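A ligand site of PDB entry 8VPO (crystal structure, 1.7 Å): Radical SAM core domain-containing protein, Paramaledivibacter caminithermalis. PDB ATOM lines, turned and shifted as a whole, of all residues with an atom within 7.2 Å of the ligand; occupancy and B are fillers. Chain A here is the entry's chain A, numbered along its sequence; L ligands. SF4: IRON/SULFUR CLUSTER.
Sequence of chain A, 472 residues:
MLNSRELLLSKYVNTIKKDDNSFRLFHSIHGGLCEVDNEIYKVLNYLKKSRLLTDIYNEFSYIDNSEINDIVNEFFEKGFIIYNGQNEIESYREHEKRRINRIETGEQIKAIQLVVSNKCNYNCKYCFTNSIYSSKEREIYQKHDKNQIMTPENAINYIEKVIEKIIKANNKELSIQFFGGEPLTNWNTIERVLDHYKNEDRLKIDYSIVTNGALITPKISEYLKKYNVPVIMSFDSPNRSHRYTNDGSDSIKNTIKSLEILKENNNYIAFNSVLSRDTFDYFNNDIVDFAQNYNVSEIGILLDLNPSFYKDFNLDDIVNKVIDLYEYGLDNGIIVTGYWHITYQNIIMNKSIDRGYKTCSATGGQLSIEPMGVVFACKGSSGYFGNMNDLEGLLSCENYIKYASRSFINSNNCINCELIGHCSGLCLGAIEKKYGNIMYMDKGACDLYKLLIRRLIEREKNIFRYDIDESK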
ATOM      1  N   LYS A 358      27.833 -31.249  21.739  1.00  0.00           N
ATOM      2  CA  LYS A 358      26.919 -31.469  20.626  1.00  0.00           C
ATOM      3  C   LYS A 358      27.714 -31.570  19.331  1.00  0.00           C
ATOM      4  O   LYS A 358      28.358 -32.603  19.092  1.00  0.00           O
ATOM      5  CB  LYS A 358      25.889 -30.330  20.639  1.00  0.00           C
ATOM      6  CG  LYS A 358      25.021 -30.457  21.907  1.00  0.00           C
ATOM      7  CD  LYS A 358      23.921 -29.302  21.972  1.00  0.00           C
ATOM      8  CE  LYS A 358      24.663 -28.029  22.211  1.00  0.00           C
ATOM      9  NZ  LYS A 358      23.600 -26.976  22.519  1.00  0.00           N
ATOM     10  N   ARG A 406      29.696 -23.877  28.289  1.00  0.00           N
ATOM     11  CA  ARG A 406      28.558 -23.727  27.387  1.00  0.00           C
ATOM     12  C   ARG A 406      28.495 -24.884  26.382  1.00  0.00           C
ATOM     13  O   ARG A 406      28.229 -24.708  25.184  1.00  0.00           O
ATOM     14  CB  ARG A 406      28.563 -22.383  26.674  1.00  0.00           C
ATOM     15  CG  ARG A 406      29.911 -22.024  25.931  1.00  0.00           C
ATOM     16  CD  ARG A 406      29.640 -21.464  24.542  1.00  0.00           C
ATOM     17  NE  ARG A 406      29.098 -22.529  23.659  1.00  0.00           N
ATOM     18  CZ  ARG A 406      28.831 -22.342  22.380  1.00  0.00           C
ATOM     19  NH1 ARG A 406      28.998 -21.150  21.802  1.00  0.00           N
ATOM     20  NH2 ARG A 406      28.375 -23.391  21.656  1.00  0.00           N
ATOM     21  N   ASN A 410      24.232 -23.462  24.703  1.00  0.00           N
ATOM     22  CA  ASN A 410      25.219 -22.533  24.136  1.00  0.00           C
ATOM     23  C   ASN A 410      25.112 -21.186  24.776  1.00  0.00           C
ATOM     24  O   ASN A 410      26.100 -20.470  24.831  1.00  0.00           O
ATOM     25  CB  ASN A 410      25.009 -22.346  22.635  1.00  0.00           C
ATOM     26  CG  ASN A 410      24.789 -23.652  21.908  1.00  0.00           C
ATOM     27  OD1 ASN A 410      25.284 -24.752  22.331  1.00  0.00           O
ATOM     28  ND2 ASN A 410      24.046 -23.580  20.731  1.00  0.00           N
ATOM     29  N   SER A 411      23.897 -20.822  25.200  1.00  0.00           N
ATOM     30  CA  SER A 411      23.611 -19.447  25.539  1.00  0.00           C
ATOM     31  C   SER A 411      22.212 -19.423  26.131  1.00  0.00           C
ATOM     32  O   SER A 411      21.376 -20.215  25.730  1.00  0.00           O
ATOM     33  CB  SER A 411      23.654 -18.615  24.251  1.00  0.00           C
ATOM     34  OG  SER A 411      23.177 -17.312  24.486  1.00  0.00           O
ATOM     35  N   ASN A 413      20.256 -17.431  25.023  1.00  0.00           N
ATOM     36  CA  ASN A 413      19.527 -17.211  23.789  1.00  0.00           C
ATOM     37  C   ASN A 413      18.798 -18.486  23.331  1.00  0.00           C
ATOM     38  O   ASN A 413      17.825 -18.399  22.567  1.00  0.00           O
ATOM     39  CB  ASN A 413      20.467 -16.846  22.591  1.00  0.00           C
ATOM     40  CG  ASN A 413      21.260 -15.544  22.759  1.00  0.00           C
ATOM     41  OD1 ASN A 413      22.401 -15.379  22.169  1.00  0.00           O
ATOM     42  ND2 ASN A 413      20.672 -14.578  23.505  1.00  0.00           N
ATOM     43  N   CYS A 414      19.272 -19.649  23.784  1.00  0.00           N
ATOM     44  CA  CYS A 414      18.841 -20.949  23.200  1.00  0.00           C
ATOM     45  C   CYS A 414      17.687 -21.604  23.947  1.00  0.00           C
ATOM     46  O   CYS A 414      17.139 -22.590  23.453  1.00  0.00           O
ATOM     47  CB  CYS A 414      19.974 -21.980  23.221  1.00  0.00           C
ATOM     48  SG  CYS A 414      21.437 -21.411  22.255  1.00  0.00           S
ATOM     49  N   ILE A 415      17.259 -21.066  25.091  1.00  0.00           N
ATOM     50  CA  ILE A 415      16.447 -21.883  25.976  1.00  0.00           C
ATOM     51  C   ILE A 415      15.112 -22.273  25.330  1.00  0.00           C
ATOM     52  O   ILE A 415      14.617 -23.384  25.569  1.00  0.00           O
ATOM     53  CB  ILE A 415      16.228 -21.173  27.314  1.00  0.00           C
ATOM     54  CG1 ILE A 415      17.582 -20.871  27.954  1.00  0.00           C
ATOM     55  CG2 ILE A 415      15.302 -22.045  28.251  1.00  0.00           C
ATOM     56  CD1 ILE A 415      18.333 -22.062  28.306  1.00  0.00           C
ATOM     57  N   ASN A 416      14.505 -21.397  24.566  1.00  0.00           N
ATOM     58  CA  ASN A 416      13.228 -21.722  23.971  1.00  0.00           C
ATOM     59  C   ASN A 416      13.361 -22.183  22.514  1.00  0.00           C
ATOM     60  O   ASN A 416      12.363 -22.223  21.789  1.00  0.00           O
ATOM     61  CB  ASN A 416      12.311 -20.519  24.060  1.00  0.00           C
ATOM     62  CG  ASN A 416      11.932 -20.200  25.534  1.00  0.00           C
ATOM     63  OD1 ASN A 416      11.812 -21.112  26.331  1.00  0.00           O
ATOM     64  ND2 ASN A 416      11.829 -18.956  25.868  1.00  0.00           N
ATOM     65  N   CYS A 417      14.587 -22.465  22.067  1.00  0.00           N
ATOM     66  CA  CYS A 417      14.806 -22.866  20.671  1.00  0.00           C
ATOM     67  C   CYS A 417      14.567 -24.388  20.468  1.00  0.00           C
ATOM     68  O   CYS A 417      14.981 -25.200  21.293  1.00  0.00           O
ATOM     69  CB  CYS A 417      16.242 -22.574  20.314  1.00  0.00           C
ATOM     70  SG  CYS A 417      16.559 -22.891  18.528  1.00  0.00           S
ATOM     71  N   GLU A 418      13.954 -24.724  19.327  1.00  0.00           N
ATOM     72  CA  GLU A 418      13.722 -26.142  19.063  1.00  0.00           C
ATOM     73  C   GLU A 418      15.014 -26.933  18.849  1.00  0.00           C
ATOM     74  O   GLU A 418      14.965 -28.195  18.845  1.00  0.00           O
ATOM     75  CB  GLU A 418      12.800 -26.257  17.845  1.00  0.00           C
ATOM     76  CG  GLU A 418      13.428 -25.799  16.510  1.00  0.00           C
ATOM     77  CD  GLU A 418      12.962 -24.433  16.166  1.00  0.00           C
ATOM     78  OE1 GLU A 418      12.792 -23.567  17.107  1.00  0.00           O
ATOM     79  OE2 GLU A 418      12.789 -24.247  14.954  1.00  0.00           O
ATOM     80  N   LEU A 419      16.167 -26.241  18.668  1.00  0.00           N
ATOM     81  CA  LEU A 419      17.397 -27.007  18.489  1.00  0.00           C
ATOM     82  C   LEU A 419      18.280 -27.027  19.722  1.00  0.00           C
ATOM     83  O   LEU A 419      19.438 -27.452  19.608  1.00  0.00           O
ATOM     84  CB  LEU A 419      18.201 -26.495  17.289  1.00  0.00           C
ATOM     85  CG  LEU A 419      17.458 -26.369  15.957  1.00  0.00           C
ATOM     86  CD1 LEU A 419      18.420 -25.841  14.900  1.00  0.00           C
ATOM     87  CD2 LEU A 419      16.889 -27.691  15.508  1.00  0.00           C
ATOM     88  N   ILE A 420      17.776 -26.620  20.892  1.00  0.00           N
ATOM     89  CA  ILE A 420      18.657 -26.356  22.028  1.00  0.00           C
ATOM     90  C   ILE A 420      19.552 -27.541  22.374  1.00  0.00           C
ATOM     91  O   ILE A 420      20.751 -27.364  22.661  1.00  0.00           O
ATOM     92  CB  ILE A 420      17.824 -25.932  23.257  1.00  0.00           C
ATOM     93  CG1 ILE A 420      18.763 -25.577  24.397  1.00  0.00           C
ATOM     94  CG2 ILE A 420      16.843 -27.054  23.678  1.00  0.00           C
ATOM     95  CD1 ILE A 420      18.055 -25.376  25.740  1.00  0.00           C
ATOM     96  N   GLY A 421      19.020 -28.779  22.288  1.00  0.00           N
ATOM     97  CA  GLY A 421      19.852 -29.905  22.688  1.00  0.00           C
ATOM     98  C   GLY A 421      20.663 -30.510  21.556  1.00  0.00           C
ATOM     99  O   GLY A 421      21.306 -31.556  21.768  1.00  0.00           O
ATOM    100  N   HIS A 422      20.668 -29.870  20.401  1.00  0.00           N
ATOM    101  CA  HIS A 422      21.197 -30.526  19.185  1.00  0.00           C
ATOM    102  C   HIS A 422      22.196 -29.668  18.459  1.00  0.00           C
ATOM    103  O   HIS A 422      22.977 -30.229  17.674  1.00  0.00           O
ATOM    104  CB  HIS A 422      20.016 -30.825  18.241  1.00  0.00           C
ATOM    105  CG  HIS A 422      18.918 -31.575  18.934  1.00  0.00           C
ATOM    106  ND1 HIS A 422      19.082 -32.862  19.410  1.00  0.00           N
ATOM    107  CD2 HIS A 422      17.662 -31.192  19.302  1.00  0.00           C
ATOM    108  CE1 HIS A 422      17.966 -33.274  19.992  1.00  0.00           C
ATOM    109  NE2 HIS A 422      17.088 -32.273  19.932  1.00  0.00           N
ATOM    110  N   CYS A 423      22.165 -28.355  18.655  1.00  0.00           N
ATOM    111  CA  CYS A 423      22.863 -27.355  17.848  1.00  0.00           C
ATOM    112  C   CYS A 423      23.849 -26.613  18.711  1.00  0.00           C
ATOM    113  O   CYS A 423      23.506 -26.236  19.839  1.00  0.00           O
ATOM    114  CB  CYS A 423      21.811 -26.365  17.332  1.00  0.00           C
ATOM    115  SG  CYS A 423      22.490 -24.833  16.600  1.00  0.00           S
ATOM    116  N   SER A 424      25.095 -26.445  18.221  1.00  0.00           N
ATOM    117  CA  SER A 424      26.123 -25.705  18.966  1.00  0.00           C
ATOM    118  C   SER A 424      26.273 -24.266  18.498  1.00  0.00           C
ATOM    119  O   SER A 424      27.157 -23.543  19.005  1.00  0.00           O
ATOM    120  CB  SER A 424      27.479 -26.404  18.797  1.00  0.00           C
ATOM    121  OG  SER A 424      27.505 -27.687  19.484  1.00  0.00           O
ATOM    122  N   GLY A 425      25.432 -23.833  17.595  1.00  0.00           N
ATOM    123  CA  GLY A 425      25.471 -22.477  17.066  1.00  0.00           C
ATOM    124  C   GLY A 425      26.583 -22.327  16.034  1.00  0.00           C
ATOM    125  O   GLY A 425      27.201 -23.295  15.597  1.00  0.00           O
ATOM    126  N   LEU A 426      26.824 -21.074  15.674  1.00  0.00           N
ATOM    127  CA  LEU A 426      27.897 -20.772  14.736  1.00  0.00           C
ATOM    128  C   LEU A 426      29.246 -20.945  15.424  1.00  0.00           C
ATOM    129  O   LEU A 426      29.453 -20.569  16.577  1.00  0.00           O
ATOM    130  CB  LEU A 426      27.698 -19.353  14.209  1.00  0.00           C
ATOM    131  CG  LEU A 426      28.712 -18.917  13.111  1.00  0.00           C
ATOM    132  CD1 LEU A 426      28.682 -19.799  11.845  1.00  0.00           C
ATOM    133  CD2 LEU A 426      28.484 -17.433  12.731  1.00  0.00           C
ATOM    134  N   MET A 441      24.940 -15.657  20.325  1.00  0.00           N
ATOM    135  CA  MET A 441      24.553 -16.426  19.148  1.00  0.00           C
ATOM    136  C   MET A 441      24.301 -15.522  17.942  1.00  0.00           C
ATOM    137  O   MET A 441      23.879 -14.354  18.074  1.00  0.00           O
ATOM    138  CB  MET A 441      23.315 -17.284  19.456  1.00  0.00           C
ATOM    139  CG  MET A 441      23.507 -18.419  20.478  1.00  0.00           C
ATOM    140  SD  MET A 441      24.887 -19.527  20.097  1.00  0.00           S
ATOM    141  CE  MET A 441      26.215 -18.799  21.082  1.00  0.00           C
ATOM    142  N   ASP A 442      24.630 -16.046  16.748  1.00  0.00           N
ATOM    143  CA  ASP A 442      24.491 -15.248  15.532  1.00  0.00           C
ATOM    144  C   ASP A 442      23.105 -15.507  14.976  1.00  0.00           C
ATOM    145  O   ASP A 442      22.790 -16.610  14.496  1.00  0.00           O
ATOM    146  CB  ASP A 442      25.589 -15.596  14.505  1.00  0.00           C
ATOM    147  CG  ASP A 442      25.497 -14.712  13.260  1.00  0.00           C
ATOM    148  OD1 ASP A 442      25.901 -13.505  13.357  1.00  0.00           O
ATOM    149  OD2 ASP A 442      24.955 -15.159  12.198  1.00  0.00           O
ATOM    150  N   LYS A 443      22.265 -14.480  14.974  1.00  0.00           N
ATOM    151  CA  LYS A 443      20.873 -14.700  14.573  1.00  0.00           C
ATOM    152  C   LYS A 443      20.738 -15.219  13.147  1.00  0.00           C
ATOM    153  O   LYS A 443      19.918 -16.107  12.896  1.00  0.00           O
ATOM    154  CB  LYS A 443      20.066 -13.395  14.771  1.00  0.00           C
ATOM    155  CG  LYS A 443      18.690 -13.501  14.108  1.00  0.00           C
ATOM    156  CD  LYS A 443      17.729 -12.381  14.526  1.00  0.00           C
ATOM    157  CE  LYS A 443      16.333 -12.665  14.014  1.00  0.00           C
ATOM    158  NZ  LYS A 443      16.380 -12.724  12.513  1.00  0.00           N
ATOM    159  N   ALA A 445      22.754 -17.123  11.333  1.00  0.00           N
ATOM    160  CA  ALA A 445      23.089 -18.538  11.291  1.00  0.00           C
ATOM    161  C   ALA A 445      22.008 -19.358  11.965  1.00  0.00           C
ATOM    162  O   ALA A 445      21.612 -20.424  11.457  1.00  0.00           O
ATOM    163  CB  ALA A 445      24.471 -18.806  11.964  1.00  0.00           C
ATOM    164  N   CYS A 446      21.527 -18.890  13.131  1.00  0.00           N
ATOM    165  CA  CYS A 446      20.435 -19.629  13.784  1.00  0.00           C
ATOM    166  C   CYS A 446      19.264 -19.776  12.857  1.00  0.00           C
ATOM    167  O   CYS A 446      18.627 -20.866  12.808  1.00  0.00           O
ATOM    168  CB  CYS A 446      19.972 -18.883  15.069  1.00  0.00           C
ATOM    169  SG  CYS A 446      21.262 -18.827  16.345  1.00  0.00           S
ATOM    170  N   ASP A 447      18.886 -18.689  12.157  1.00  0.00           N
ATOM    171  CA  ASP A 447      17.733 -18.805  11.256  1.00  0.00           C
ATOM    172  C   ASP A 447      17.948 -19.882  10.201  1.00  0.00           C
ATOM    173  O   ASP A 447      17.020 -20.660   9.914  1.00  0.00           O
ATOM    174  CB  ASP A 447      17.433 -17.462  10.552  1.00  0.00           C
ATOM    175  CG  ASP A 447      16.945 -16.386  11.556  1.00  0.00           C
ATOM    176  OD1 ASP A 447      16.531 -16.752  12.696  1.00  0.00           O
ATOM    177  OD2 ASP A 447      16.993 -15.179  11.169  1.00  0.00           O
ATOM    178  N   LEU A 448      19.154 -19.952   9.643  1.00  0.00           N
ATOM    179  CA  LEU A 448      19.465 -20.988   8.643  1.00  0.00           C
ATOM    180  C   LEU A 448      19.386 -22.378   9.271  1.00  0.00           C
ATOM    181  O   LEU A 448      18.797 -23.309   8.678  1.00  0.00           O
ATOM    182  CB  LEU A 448      20.867 -20.708   8.103  1.00  0.00           C
ATOM    183  CG  LEU A 448      21.362 -21.609   6.954  1.00  0.00           C
ATOM    184  CD1 LEU A 448      21.945 -22.867   7.537  1.00  0.00           C
ATOM    185  CD2 LEU A 448      20.243 -21.923   5.917  1.00  0.00           C
ATOM    186  N   TYR A 449      19.975 -22.547  10.471  1.00  0.00           N
ATOM    187  CA  TYR A 449      19.948 -23.883  11.066  1.00  0.00           C
ATOM    188  C   TYR A 449      18.530 -24.381  11.239  1.00  0.00           C
ATOM    189  O   TYR A 449      18.244 -25.578  11.028  1.00  0.00           O
ATOM    190  CB  TYR A 449      20.661 -23.926  12.433  1.00  0.00           C
ATOM    191  CG  TYR A 449      22.116 -23.452  12.387  1.00  0.00           C
ATOM    192  CD1 TYR A 449      22.897 -23.650  11.203  1.00  0.00           C
ATOM    193  CD2 TYR A 449      22.673 -22.784  13.484  1.00  0.00           C
ATOM    194  CE1 TYR A 449      24.236 -23.247  11.176  1.00  0.00           C
ATOM    195  CE2 TYR A 449      24.005 -22.331  13.470  1.00  0.00           C
ATOM    196  CZ  TYR A 449      24.752 -22.533  12.292  1.00  0.00           C
ATOM    197  OH  TYR A 449      26.062 -22.117  12.322  1.00  0.00           O
ATOM    198  N   LYS A 450      17.663 -23.510  11.755  1.00  0.00           N
ATOM    199  CA  LYS A 450      16.273 -23.893  11.968  1.00  0.00           C
ATOM    200  C   LYS A 450      15.574 -24.243  10.668  1.00  0.00           C
ATOM    201  O   LYS A 450      14.859 -25.240  10.613  1.00  0.00           O
ATOM    202  CB  LYS A 450      15.567 -22.757  12.735  1.00  0.00           C
ATOM    203  CG  LYS A 450      16.108 -22.740  14.193  1.00  0.00           C
ATOM    204  CD  LYS A 450      15.363 -21.708  15.080  1.00  0.00           C
ATOM    205  CE  LYS A 450      16.041 -20.414  15.116  1.00  0.00           C
ATOM    206  NZ  LYS A 450      15.054 -19.457  15.800  1.00  0.00           N
HETATM  207 FE1  SF4 L   1      21.269 -23.259  17.768  1.00  0.00          FE
HETATM  208 FE2  SF4 L   1      20.849 -21.735  20.016  1.00  0.00          FE
HETATM  209 FE3  SF4 L   1      18.792 -22.411  18.443  1.00  0.00          FE
HETATM  210 FE4  SF4 L   1      20.607 -20.631  17.602  1.00  0.00          FE
HETATM  211  S1  SF4 L   1      19.200 -20.338  19.325  1.00  0.00           S
HETATM  212  S2  SF4 L   1      19.690 -22.315  16.377  1.00  0.00           S
HETATM  213  S3  SF4 L   1      22.491 -21.483  18.539  1.00  0.00           S
HETATM  214  S4  SF4 L   1      20.089 -23.864  19.586  1.00  0.00           S
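The side-chain sulfur (SG) of Cys 417 is bound to an iron atom (FE3) of the ligand (2.3 Å). The side-chain sulfur (SG) of Cys 446 is bound to an iron atom (FE4) of the ligand (2.3 Å). SG of Cys 423 is bound to FE1 of the ligand (2.3 Å). SG of Cys 414 binds FE2 of the ligand. ND2 of Asn 410 sits close to S3 of the ligand, at 3.4 Å.
ND2 of Asn 410 sits at hydrogen-bond distance from O of Cys 423. The backbone carbonyl oxygen (O) of Cys 423 is in hydrogen-bond range of the side-chain amino group (NZ) of Lys 358 (2.8 Å). The side-chain sulfur of Cys 414 lies close to the side-chain amide nitrogen of Asn 410 (3.7 Å). SG of Cys 414 sits close to O of Ser 411 (3.7 Å). The side-chain amide nitrogen of Asn 410 sits close to the backbone NH of Gly 425. NZ of Lys 358 lies within hydrogen-bond range of OD1 of Asn 410, 2.8 Å away. NH2 of Arg 406 lies within hydrogen-bond range of OD1 of Asn 410 (3.4 Å). The backbone NH (N) of Met 441 lies within hydrogen-bond range of the side-chain amide oxygen (OD1) of Asn 413.
The backbone carbonyl oxygen (O) of Leu 419 sits close to a sulfur (S4) of the ligand (3.6 Å). S3 of the ligand lies close to SD of Met 441 (3.5 Å). Residues that only touch the ligand: Gly 425 (3.5 Å) and Ile 420 (3.8 Å). Within 4 Å of the ligand: Asn 410, Cys 414, Cys 417, Leu 419, Ile 420, Cys 423, Gly 425, Met 441 and Cys 446.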
